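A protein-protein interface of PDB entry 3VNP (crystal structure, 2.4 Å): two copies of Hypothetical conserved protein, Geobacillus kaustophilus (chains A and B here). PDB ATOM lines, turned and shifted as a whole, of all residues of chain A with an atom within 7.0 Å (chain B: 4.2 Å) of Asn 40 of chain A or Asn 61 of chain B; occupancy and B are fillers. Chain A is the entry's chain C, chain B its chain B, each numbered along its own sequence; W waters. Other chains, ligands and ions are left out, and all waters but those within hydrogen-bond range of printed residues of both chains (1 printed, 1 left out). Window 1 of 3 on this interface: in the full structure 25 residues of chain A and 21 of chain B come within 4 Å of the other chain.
Water W1 lies within hydrogen-bond range of the side-chain amide nitrogen of Gln 83 of chain B, the backbone carbonyl oxygen of Asn 61 of chain A and the side-chain amide oxygen of Asn 61 of chain B.
Of the 17 printed residues of chain A, 8 touch a printed residue of chain B. Printed residues of chain A that touch a printed residue of chain B: Tyr 22, Thr 24, Asn 40, Val 42, Asn 61, Ser 62, Ile 63 and Gln 83. Hydrophobic or aromatic side chains of chain A that line the printed part of chain B: Val 42 and Ile 63. Among the printed residues, no Asp or Glu carboxylate lies within 4 Å of a Lys or Arg side-chain nitrogen of the other chain.
Asn 40 of chain A touches its own counterpart, Asn 40 of chain B. Asn 61 of chain B touches its own counterpart, Asn 61 of chain A. Asn 61 of chain A touches Gln 83 of chain B, but with the chains exchanged Gln 83 of chain A does not touch Asn 61 of chain B (6.6 Å). Ser 62 of chain A touches Asn 61 of chain B, but with the chains exchanged Asn 61 of chain A does not touch Ser 62 of chain B (8.0 Å). Of the 15 pairs that touch across the chains among the printed residues, 3 have their exchanged pair printed and touching as well.
ND2 of Asn 40 of chain B touches O of Tyr 22 of chain A (3.9 Å). Asn 40 of chain A touches Asn 61 of chain B. CG2 of Val 42 of chain A touches CB of Phe 39 of chain B, 3.98 Å away. CG1 of Val 42 of chain A touches OD1 of Asp 60 of chain B, at 3.7 Å. ND2 of Asn 61 of chain B touches CG2 of Val 42 of chain A, 3.98 Å away. Asn 61 of chain A touches Gln 83 of chain B. Ser 62 of chain A touches Asn 61 of chain B. CD1 of Ile 63 of chain A touches O of Asp 60 of chain B, 3.6 Å away. Ile 63 of chain A touches Asn 61 of chain B (CG1 to ND2, 3.4 Å). Ile 63 of chain A touches Gln 83 of chain B (CD1 to CB, 3.4 Å).
N of Val 42 of chain A lies within hydrogen-bond range of O of Ser 62 of chain A, at 2.8 Å. The backbone carbonyl oxygen (O) of Gln 59 of chain A is in hydrogen-bond range of the side-chain hydroxyl (OG) of Ser 62 of chain A (2.9 Å). The backbone carbonyl oxygen (O) of Asp 21 of chain A is in hydrogen-bond range of the backbone NH (N) of Asn 40 of chain A, at 3.3 Å. N of Gln 83 of chain B is in hydrogen-bond range of O of Asp 60 of chain B. The backbone NH (N) of Asn 61 of chain B sits at hydrogen-bond distance from the backbone carbonyl oxygen (O) of Phe 39 of chain B, at 2.8 Å. The backbone NH of Gln 83 of chain A lies within hydrogen-bond range of the backbone carbonyl oxygen of Asp 60 of chain A, at 2.8 Å.
The side-chain amide oxygen of Asn 40 of chain B sits close to the side-chain amide oxygen of Asn 40 of chain A. The side-chain amide oxygen of Asn 61 of chain A sits close to the side-chain amide oxygen of Asn 61 of chain B (3.1 Å).
Val 23 of chain A touches none of the printed residues of chain B. Phe 39 of chain A touches none of the printed residues of chain B. Of the printed residues of chain B, Asn 61 of chain A touches Asn 61 and Gln 83. Printed residues of chain B within 4 Å of Ser 62 of chain A: Asn 61 (3.98 Å). Of the printed residues of chain B, Ile 63 of chain A touches Asp 60 (3.6 Å), Asn 61 (3.4 Å) and Gln 83 (3.4 Å). Printed residues of chain A within 4 Å of Phe 39 of chain B: Thr 24 and Val 42. Of the printed residues of chain A, Asn 61 of chain B touches Asn 40, Val 42, Asn 61, Ser 62 and Ile 63. The nearest printed residue of chain B that does not touch Asn 40 of chain A is Phe 39 of chain B (6.7 Å).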
ATOM      1  N   ALA A  20      -0.632 -18.383  12.780  1.00  0.00           N
ATOM      2  CA  ALA A  20      -1.004 -17.074  12.253  1.00  0.00           C
ATOM      3  C   ALA A  20       0.157 -16.420  11.515  1.00  0.00           C
ATOM      4  O   ALA A  20       1.279 -16.927  11.525  1.00  0.00           O
ATOM      5  CB  ALA A  20      -1.459 -16.178  13.390  1.00  0.00           C
ATOM      6  N   ASP A  21      -0.115 -15.282  10.884  1.00  0.00           N
ATOM      7  CA  ASP A  21       0.911 -14.551  10.147  1.00  0.00           C
ATOM      8  C   ASP A  21       1.827 -13.789  11.087  1.00  0.00           C
ATOM      9  O   ASP A  21       1.481 -13.533  12.236  1.00  0.00           O
ATOM     10  CB  ASP A  21       0.271 -13.553   9.178  1.00  0.00           C
ATOM     11  CG  ASP A  21      -0.663 -14.215   8.196  1.00  0.00           C
ATOM     12  OD1 ASP A  21      -0.204 -15.058   7.397  1.00  0.00           O
ATOM     13  OD2 ASP A  21      -1.865 -13.889   8.227  1.00  0.00           O
ATOM     14  N   TYR A  22       2.993 -13.425  10.574  1.00  0.00           N
ATOM     15  CA  TYR A  22       3.989 -12.668  11.325  1.00  0.00           C
ATOM     16  C   TYR A  22       4.435 -13.386  12.587  1.00  0.00           C
ATOM     17  O   TYR A  22       4.911 -12.767  13.535  1.00  0.00           O
ATOM     18  CB  TYR A  22       3.442 -11.276  11.663  1.00  0.00           C
ATOM     19  CG  TYR A  22       2.854 -10.554  10.463  1.00  0.00           C
ATOM     20  CD1 TYR A  22       3.551 -10.489   9.256  1.00  0.00           C
ATOM     21  CD2 TYR A  22       1.613  -9.916  10.544  1.00  0.00           C
ATOM     22  CE1 TYR A  22       3.032  -9.807   8.159  1.00  0.00           C
ATOM     23  CE2 TYR A  22       1.084  -9.230   9.452  1.00  0.00           C
ATOM     24  CZ  TYR A  22       1.804  -9.177   8.263  1.00  0.00           C
ATOM     25  OH  TYR A  22       1.316  -8.467   7.186  1.00  0.00           O
ATOM     26  N   VAL A  23       4.257 -14.701  12.602  1.00  0.00           N
ATOM     27  CA  VAL A  23       4.691 -15.510  13.727  1.00  0.00           C
ATOM     28  C   VAL A  23       6.093 -16.005  13.378  1.00  0.00           C
ATOM     29  O   VAL A  23       6.434 -16.165  12.207  1.00  0.00           O
ATOM     30  CB  VAL A  23       3.752 -16.722  13.954  1.00  0.00           C
ATOM     31  CG1 VAL A  23       4.404 -17.725  14.893  1.00  0.00           C
ATOM     32  CG2 VAL A  23       2.427 -16.253  14.551  1.00  0.00           C
ATOM     33  N   THR A  24       6.903 -16.227  14.402  1.00  0.00           N
ATOM     34  CA  THR A  24       8.267 -16.702  14.235  1.00  0.00           C
ATOM     35  C   THR A  24       8.480 -17.854  15.199  1.00  0.00           C
ATOM     36  O   THR A  24       8.300 -17.704  16.404  1.00  0.00           O
ATOM     37  CB  THR A  24       9.282 -15.597  14.582  1.00  0.00           C
ATOM     38  OG1 THR A  24       9.103 -14.494  13.690  1.00  0.00           O
ATOM     39  CG2 THR A  24      10.704 -16.110  14.470  1.00  0.00           C
ATOM     40  N   ILE A  37      -1.326 -20.641  17.261  1.00  0.00           N
ATOM     41  CA  ILE A  37      -0.327 -19.633  17.599  1.00  0.00           C
ATOM     42  C   ILE A  37      -0.796 -18.370  16.891  1.00  0.00           C
ATOM     43  O   ILE A  37      -0.765 -18.295  15.666  1.00  0.00           O
ATOM     44  CB  ILE A  37       1.064 -20.057  17.069  1.00  0.00           C
ATOM     45  CG1 ILE A  37       1.382 -21.488  17.528  1.00  0.00           C
ATOM     46  CG2 ILE A  37       2.131 -19.082  17.543  1.00  0.00           C
ATOM     47  CD1 ILE A  37       1.390 -21.688  19.033  1.00  0.00           C
ATOM     48  N   TRP A  38      -1.228 -17.373  17.655  1.00  0.00           N
ATOM     49  CA  TRP A  38      -1.754 -16.164  17.040  1.00  0.00           C
ATOM     50  C   TRP A  38      -0.762 -15.091  16.623  1.00  0.00           C
ATOM     51  O   TRP A  38       0.407 -15.126  16.993  1.00  0.00           O
ATOM     52  CB  TRP A  38      -2.871 -15.597  17.918  1.00  0.00           C
ATOM     53  CG  TRP A  38      -3.985 -16.592  18.027  1.00  0.00           C
ATOM     54  CD1 TRP A  38      -4.034 -17.682  18.855  1.00  0.00           C
ATOM     55  CD2 TRP A  38      -5.127 -16.694  17.167  1.00  0.00           C
ATOM     56  NE1 TRP A  38      -5.126 -18.459  18.556  1.00  0.00           N
ATOM     57  CE2 TRP A  38      -5.815 -17.879  17.524  1.00  0.00           C
ATOM     58  CE3 TRP A  38      -5.634 -15.906  16.124  1.00  0.00           C
ATOM     59  CZ2 TRP A  38      -6.985 -18.297  16.869  1.00  0.00           C
ATOM     60  CZ3 TRP A  38      -6.799 -16.319  15.469  1.00  0.00           C
ATOM     61  CH2 TRP A  38      -7.459 -17.504  15.845  1.00  0.00           C
ATOM     62  N   PHE A  39      -1.264 -14.155  15.822  1.00  0.00           N
ATOM     63  CA  PHE A  39      -0.502 -13.055  15.233  1.00  0.00           C
ATOM     64  C   PHE A  39       0.657 -12.404  15.976  1.00  0.00           C
ATOM     65  O   PHE A  39       0.537 -12.005  17.127  1.00  0.00           O
ATOM     66  CB  PHE A  39      -1.481 -11.969  14.777  1.00  0.00           C
ATOM     67  CG  PHE A  39      -2.451 -12.440  13.724  1.00  0.00           C
ATOM     68  CD1 PHE A  39      -2.037 -12.597  12.399  1.00  0.00           C
ATOM     69  CD2 PHE A  39      -3.758 -12.804  14.073  1.00  0.00           C
ATOM     70  CE1 PHE A  39      -2.905 -13.116  11.436  1.00  0.00           C
ATOM     71  CE2 PHE A  39      -4.633 -13.324  13.121  1.00  0.00           C
ATOM     72  CZ  PHE A  39      -4.208 -13.483  11.796  1.00  0.00           C
ATOM     73  N   ASN A  40       1.785 -12.300  15.275  1.00  0.00           N
ATOM     74  CA  ASN A  40       2.996 -11.668  15.787  1.00  0.00           C
ATOM     75  C   ASN A  40       3.633 -12.339  16.993  1.00  0.00           C
ATOM     76  O   ASN A  40       4.474 -11.745  17.663  1.00  0.00           O
ATOM     77  CB  ASN A  40       2.699 -10.199  16.101  1.00  0.00           C
ATOM     78  CG  ASN A  40       2.510  -9.366  14.845  1.00  0.00           C
ATOM     79  OD1 ASN A  40       3.460  -8.779  14.320  1.00  0.00           O
ATOM     80  ND2 ASN A  40       1.289  -9.330  14.344  1.00  0.00           N
ATOM     81  N   THR A  41       3.247 -13.577  17.277  1.00  0.00           N
ATOM     82  CA  THR A  41       3.826 -14.283  18.412  1.00  0.00           C
ATOM     83  C   THR A  41       5.216 -14.845  18.081  1.00  0.00           C
ATOM     84  O   THR A  41       5.456 -15.346  16.979  1.00  0.00           O
ATOM     85  CB  THR A  41       2.885 -15.418  18.891  1.00  0.00           C
ATOM     86  OG1 THR A  41       1.764 -14.839  19.570  1.00  0.00           O
ATOM     87  CG2 THR A  41       3.602 -16.372  19.840  1.00  0.00           C
ATOM     88  N   VAL A  42       6.136 -14.742  19.037  1.00  0.00           N
ATOM     89  CA  VAL A  42       7.492 -15.242  18.840  1.00  0.00           C
ATOM     90  C   VAL A  42       7.817 -16.399  19.780  1.00  0.00           C
ATOM     91  O   VAL A  42       7.599 -16.318  20.989  1.00  0.00           O
ATOM     92  CB  VAL A  42       8.543 -14.124  19.057  1.00  0.00           C
ATOM     93  CG1 VAL A  42       9.949 -14.702  18.969  1.00  0.00           C
ATOM     94  CG2 VAL A  42       8.363 -13.043  18.019  1.00  0.00           C
ATOM     95  N   GLN A  59      -2.184 -16.688  22.430  1.00  0.00           N
ATOM     96  CA  GLN A  59      -2.717 -15.484  21.840  1.00  0.00           C
ATOM     97  C   GLN A  59      -1.682 -14.483  21.327  1.00  0.00           C
ATOM     98  O   GLN A  59      -0.486 -14.586  21.618  1.00  0.00           O
ATOM     99  CB  GLN A  59      -3.722 -14.859  22.807  1.00  0.00           C
ATOM    100  CG  GLN A  59      -5.062 -15.592  22.743  1.00  0.00           C
ATOM    101  CD  GLN A  59      -5.979 -15.307  23.920  1.00  0.00           C
ATOM    102  OE1 GLN A  59      -6.250 -14.151  24.260  1.00  0.00           O
ATOM    103  NE2 GLN A  59      -6.477 -16.374  24.543  1.00  0.00           N
ATOM    104  N   ASP A  60      -2.177 -13.539  20.529  1.00  0.00           N
ATOM    105  CA  ASP A  60      -1.404 -12.496  19.846  1.00  0.00           C
ATOM    106  C   ASP A  60      -0.275 -11.783  20.584  1.00  0.00           C
ATOM    107  O   ASP A  60      -0.415 -11.394  21.736  1.00  0.00           O
ATOM    108  CB  ASP A  60      -2.376 -11.441  19.318  1.00  0.00           C
ATOM    109  CG  ASP A  60      -3.692 -12.043  18.867  1.00  0.00           C
ATOM    110  OD1 ASP A  60      -3.810 -12.425  17.685  1.00  0.00           O
ATOM    111  OD2 ASP A  60      -4.603 -12.149  19.710  1.00  0.00           O
ATOM    112  N   ASN A  61       0.839 -11.595  19.886  1.00  0.00           N
ATOM    113  CA  ASN A  61       1.997 -10.895  20.432  1.00  0.00           C
ATOM    114  C   ASN A  61       2.619 -11.473  21.689  1.00  0.00           C
ATOM    115  O   ASN A  61       3.028 -10.732  22.577  1.00  0.00           O
ATOM    116  CB  ASN A  61       1.647  -9.431  20.696  1.00  0.00           C
ATOM    117  CG  ASN A  61       2.029  -8.538  19.559  1.00  0.00           C
ATOM    118  OD1 ASN A  61       3.209  -8.432  19.206  1.00  0.00           O
ATOM    119  ND2 ASN A  61       1.039  -7.885  18.963  1.00  0.00           N
ATOM    120  N   SER A  62       2.696 -12.788  21.784  1.00  0.00           N
ATOM    121  CA  SER A  62       3.319 -13.365  22.960  1.00  0.00           C
ATOM    122  C   SER A  62       4.772 -13.707  22.644  1.00  0.00           C
ATOM    123  O   SER A  62       5.175 -13.750  21.480  1.00  0.00           O
ATOM    124  CB  SER A  62       2.564 -14.613  23.412  1.00  0.00           C
ATOM    125  OG  SER A  62       1.270 -14.266  23.860  1.00  0.00           O
ATOM    126  N   ILE A  63       5.550 -13.930  23.697  1.00  0.00           N
ATOM    127  CA  ILE A  63       6.956 -14.279  23.573  1.00  0.00           C
ATOM    128  C   ILE A  63       7.224 -15.493  24.444  1.00  0.00           C
ATOM    129  O   ILE A  63       6.939 -15.486  25.643  1.00  0.00           O
ATOM    130  CB  ILE A  63       7.870 -13.151  24.071  1.00  0.00           C
ATOM    131  CG1 ILE A  63       7.500 -11.847  23.389  1.00  0.00           C
ATOM    132  CG2 ILE A  63       9.331 -13.501  23.793  1.00  0.00           C
ATOM    133  CD1 ILE A  63       8.161 -10.659  24.032  1.00  0.00           C
ATOM    134  N   GLN A  83      -0.147 -10.823  24.443  1.00  0.00           N
ATOM    135  CA  GLN A  83       1.057 -10.229  25.003  1.00  0.00           C
ATOM    136  C   GLN A  83       1.564 -10.855  26.288  1.00  0.00           C
ATOM    137  O   GLN A  83       1.820 -10.149  27.258  1.00  0.00           O
ATOM    138  CB  GLN A  83       0.791  -8.759  25.276  1.00  0.00           C
ATOM    139  CG  GLN A  83       1.653  -7.806  24.523  1.00  0.00           C
ATOM    140  CD  GLN A  83       1.363  -6.391  24.946  1.00  0.00           C
ATOM    141  OE1 GLN A  83       1.492  -6.049  26.126  1.00  0.00           O
ATOM    142  NE2 GLN A  83       0.955  -5.558  23.996  1.00  0.00           N
ATOM    143  N   PHE B  39      13.383 -10.281  16.453  1.00  0.00           N
ATOM    144  CA  PHE B  39      12.038 -10.374  15.892  1.00  0.00           C
ATOM    145  C   PHE B  39      10.940  -9.457  16.412  1.00  0.00           C
ATOM    146  O   PHE B  39      10.745  -9.307  17.620  1.00  0.00           O
ATOM    147  CB  PHE B  39      11.563 -11.821  15.986  1.00  0.00           C
ATOM    148  CG  PHE B  39      12.438 -12.784  15.246  1.00  0.00           C
ATOM    149  CD1 PHE B  39      12.368 -12.883  13.860  1.00  0.00           C
ATOM    150  CD2 PHE B  39      13.373 -13.560  15.930  1.00  0.00           C
ATOM    151  CE1 PHE B  39      13.220 -13.741  13.162  1.00  0.00           C
ATOM    152  CE2 PHE B  39      14.230 -14.419  15.240  1.00  0.00           C
ATOM    153  CZ  PHE B  39      14.152 -14.508  13.854  1.00  0.00           C
ATOM    154  N   ASN B  40      10.222  -8.858  15.460  1.00  0.00           N
ATOM    155  CA  ASN B  40       9.099  -7.965  15.728  1.00  0.00           C
ATOM    156  C   ASN B  40       9.423  -6.692  16.485  1.00  0.00           C
ATOM    157  O   ASN B  40       8.517  -6.003  16.948  1.00  0.00           O
ATOM    158  CB  ASN B  40       8.002  -8.728  16.466  1.00  0.00           C
ATOM    159  CG  ASN B  40       7.256  -9.676  15.562  1.00  0.00           C
ATOM    160  OD1 ASN B  40       6.211  -9.334  15.001  1.00  0.00           O
ATOM    161  ND2 ASN B  40       7.794 -10.871  15.394  1.00  0.00           N
ATOM    162  N   THR B  41      10.703  -6.367  16.616  1.00  0.00           N
ATOM    163  CA  THR B  41      11.070  -5.151  17.324  1.00  0.00           C
ATOM    164  C   THR B  41      10.844  -3.934  16.431  1.00  0.00           C
ATOM    165  O   THR B  41      10.980  -4.003  15.205  1.00  0.00           O
ATOM    166  CB  THR B  41      12.535  -5.207  17.808  1.00  0.00           C
ATOM    167  OG1 THR B  41      12.621  -6.103  18.918  1.00  0.00           O
ATOM    168  CG2 THR B  41      13.031  -3.834  18.244  1.00  0.00           C
ATOM    169  N   GLN B  59      16.141  -7.491  22.389  1.00  0.00           N
ATOM    170  CA  GLN B  59      15.335  -8.683  22.206  1.00  0.00           C
ATOM    171  C   GLN B  59      13.944  -8.498  21.604  1.00  0.00           C
ATOM    172  O   GLN B  59      13.429  -7.380  21.514  1.00  0.00           O
ATOM    173  CB  GLN B  59      15.295  -9.458  23.522  1.00  0.00           C
ATOM    174  CG  GLN B  59      16.657 -10.101  23.818  1.00  0.00           C
ATOM    175  CD  GLN B  59      16.749 -10.738  25.188  1.00  0.00           C
ATOM    176  OE1 GLN B  59      15.831 -11.437  25.634  1.00  0.00           O
ATOM    177  NE2 GLN B  59      17.873 -10.516  25.863  1.00  0.00           N
ATOM    178  N   ASP B  60      13.371  -9.623  21.180  1.00  0.00           N
ATOM    179  CA  ASP B  60      12.070  -9.712  20.511  1.00  0.00           C
ATOM    180  C   ASP B  60      10.915  -8.866  21.052  1.00  0.00           C
ATOM    181  O   ASP B  60      10.711  -8.766  22.258  1.00  0.00           O
ATOM    182  CB  ASP B  60      11.611 -11.182  20.471  1.00  0.00           C
ATOM    183  CG  ASP B  60      12.776 -12.176  20.541  1.00  0.00           C
ATOM    184  OD1 ASP B  60      13.126 -12.791  19.507  1.00  0.00           O
ATOM    185  OD2 ASP B  60      13.341 -12.342  21.645  1.00  0.00           O
ATOM    186  N   ASN B  61      10.151  -8.268  20.143  1.00  0.00           N
ATOM    187  CA  ASN B  61       8.982  -7.471  20.517  1.00  0.00           C
ATOM    188  C   ASN B  61       9.218  -6.201  21.319  1.00  0.00           C
ATOM    189  O   ASN B  61       8.338  -5.769  22.056  1.00  0.00           O
ATOM    190  CB  ASN B  61       7.992  -8.335  21.300  1.00  0.00           C
ATOM    191  CG  ASN B  61       6.947  -8.961  20.420  1.00  0.00           C
ATOM    192  OD1 ASN B  61       6.217  -8.258  19.711  1.00  0.00           O
ATOM    193  ND2 ASN B  61       6.849 -10.287  20.463  1.00  0.00           N
ATOM    194  N   SER B  62      10.388  -5.592  21.202  1.00  0.00           N
ATOM    195  CA  SER B  62      10.618  -4.364  21.951  1.00  0.00           C
ATOM    196  C   SER B  62      10.217  -3.171  21.109  1.00  0.00           C
ATOM    197  O   SER B  62      10.054  -3.280  19.898  1.00  0.00           O
ATOM    198  CB  SER B  62      12.088  -4.236  22.355  1.00  0.00           C
ATOM    199  OG  SER B  62      12.428  -5.229  23.301  1.00  0.00           O
ATOM    200  N   ILE B  63      10.053  -2.032  21.762  1.00  0.00           N
ATOM    201  CA  ILE B  63       9.689  -0.810  21.067  1.00  0.00           C
ATOM    202  C   ILE B  63      10.553   0.337  21.594  1.00  0.00           C
ATOM    203  O   ILE B  63      10.588   0.607  22.795  1.00  0.00           O
ATOM    204  CB  ILE B  63       8.162  -0.510  21.245  1.00  0.00           C
ATOM    205  CG1 ILE B  63       7.852   0.947  20.884  1.00  0.00           C
ATOM    206  CG2 ILE B  63       7.722  -0.863  22.650  1.00  0.00           C
ATOM    207  CD1 ILE B  63       7.934   1.240  19.386  1.00  0.00           C
ATOM    208  N   GLN B  83      10.158  -7.696  24.782  1.00  0.00           N
ATOM    209  CA  GLN B  83       9.026  -6.812  25.008  1.00  0.00           C
ATOM    210  C   GLN B  83       9.317  -5.667  25.962  1.00  0.00           C
ATOM    211  O   GLN B  83       8.579  -5.431  26.917  1.00  0.00           O
ATOM    212  CB  GLN B  83       7.883  -7.663  25.546  1.00  0.00           C
ATOM    213  CG  GLN B  83       6.496  -7.139  25.326  1.00  0.00           C
ATOM    214  CD  GLN B  83       5.493  -7.903  26.173  1.00  0.00           C
ATOM    215  OE1 GLN B  83       5.372  -7.663  27.381  1.00  0.00           O
ATOM    216  NE2 GLN B  83       4.793  -8.850  25.553  1.00  0.00           N
HETATM  217  O   HOH W   1       5.042  -8.524  22.907  1.00  0.00           O
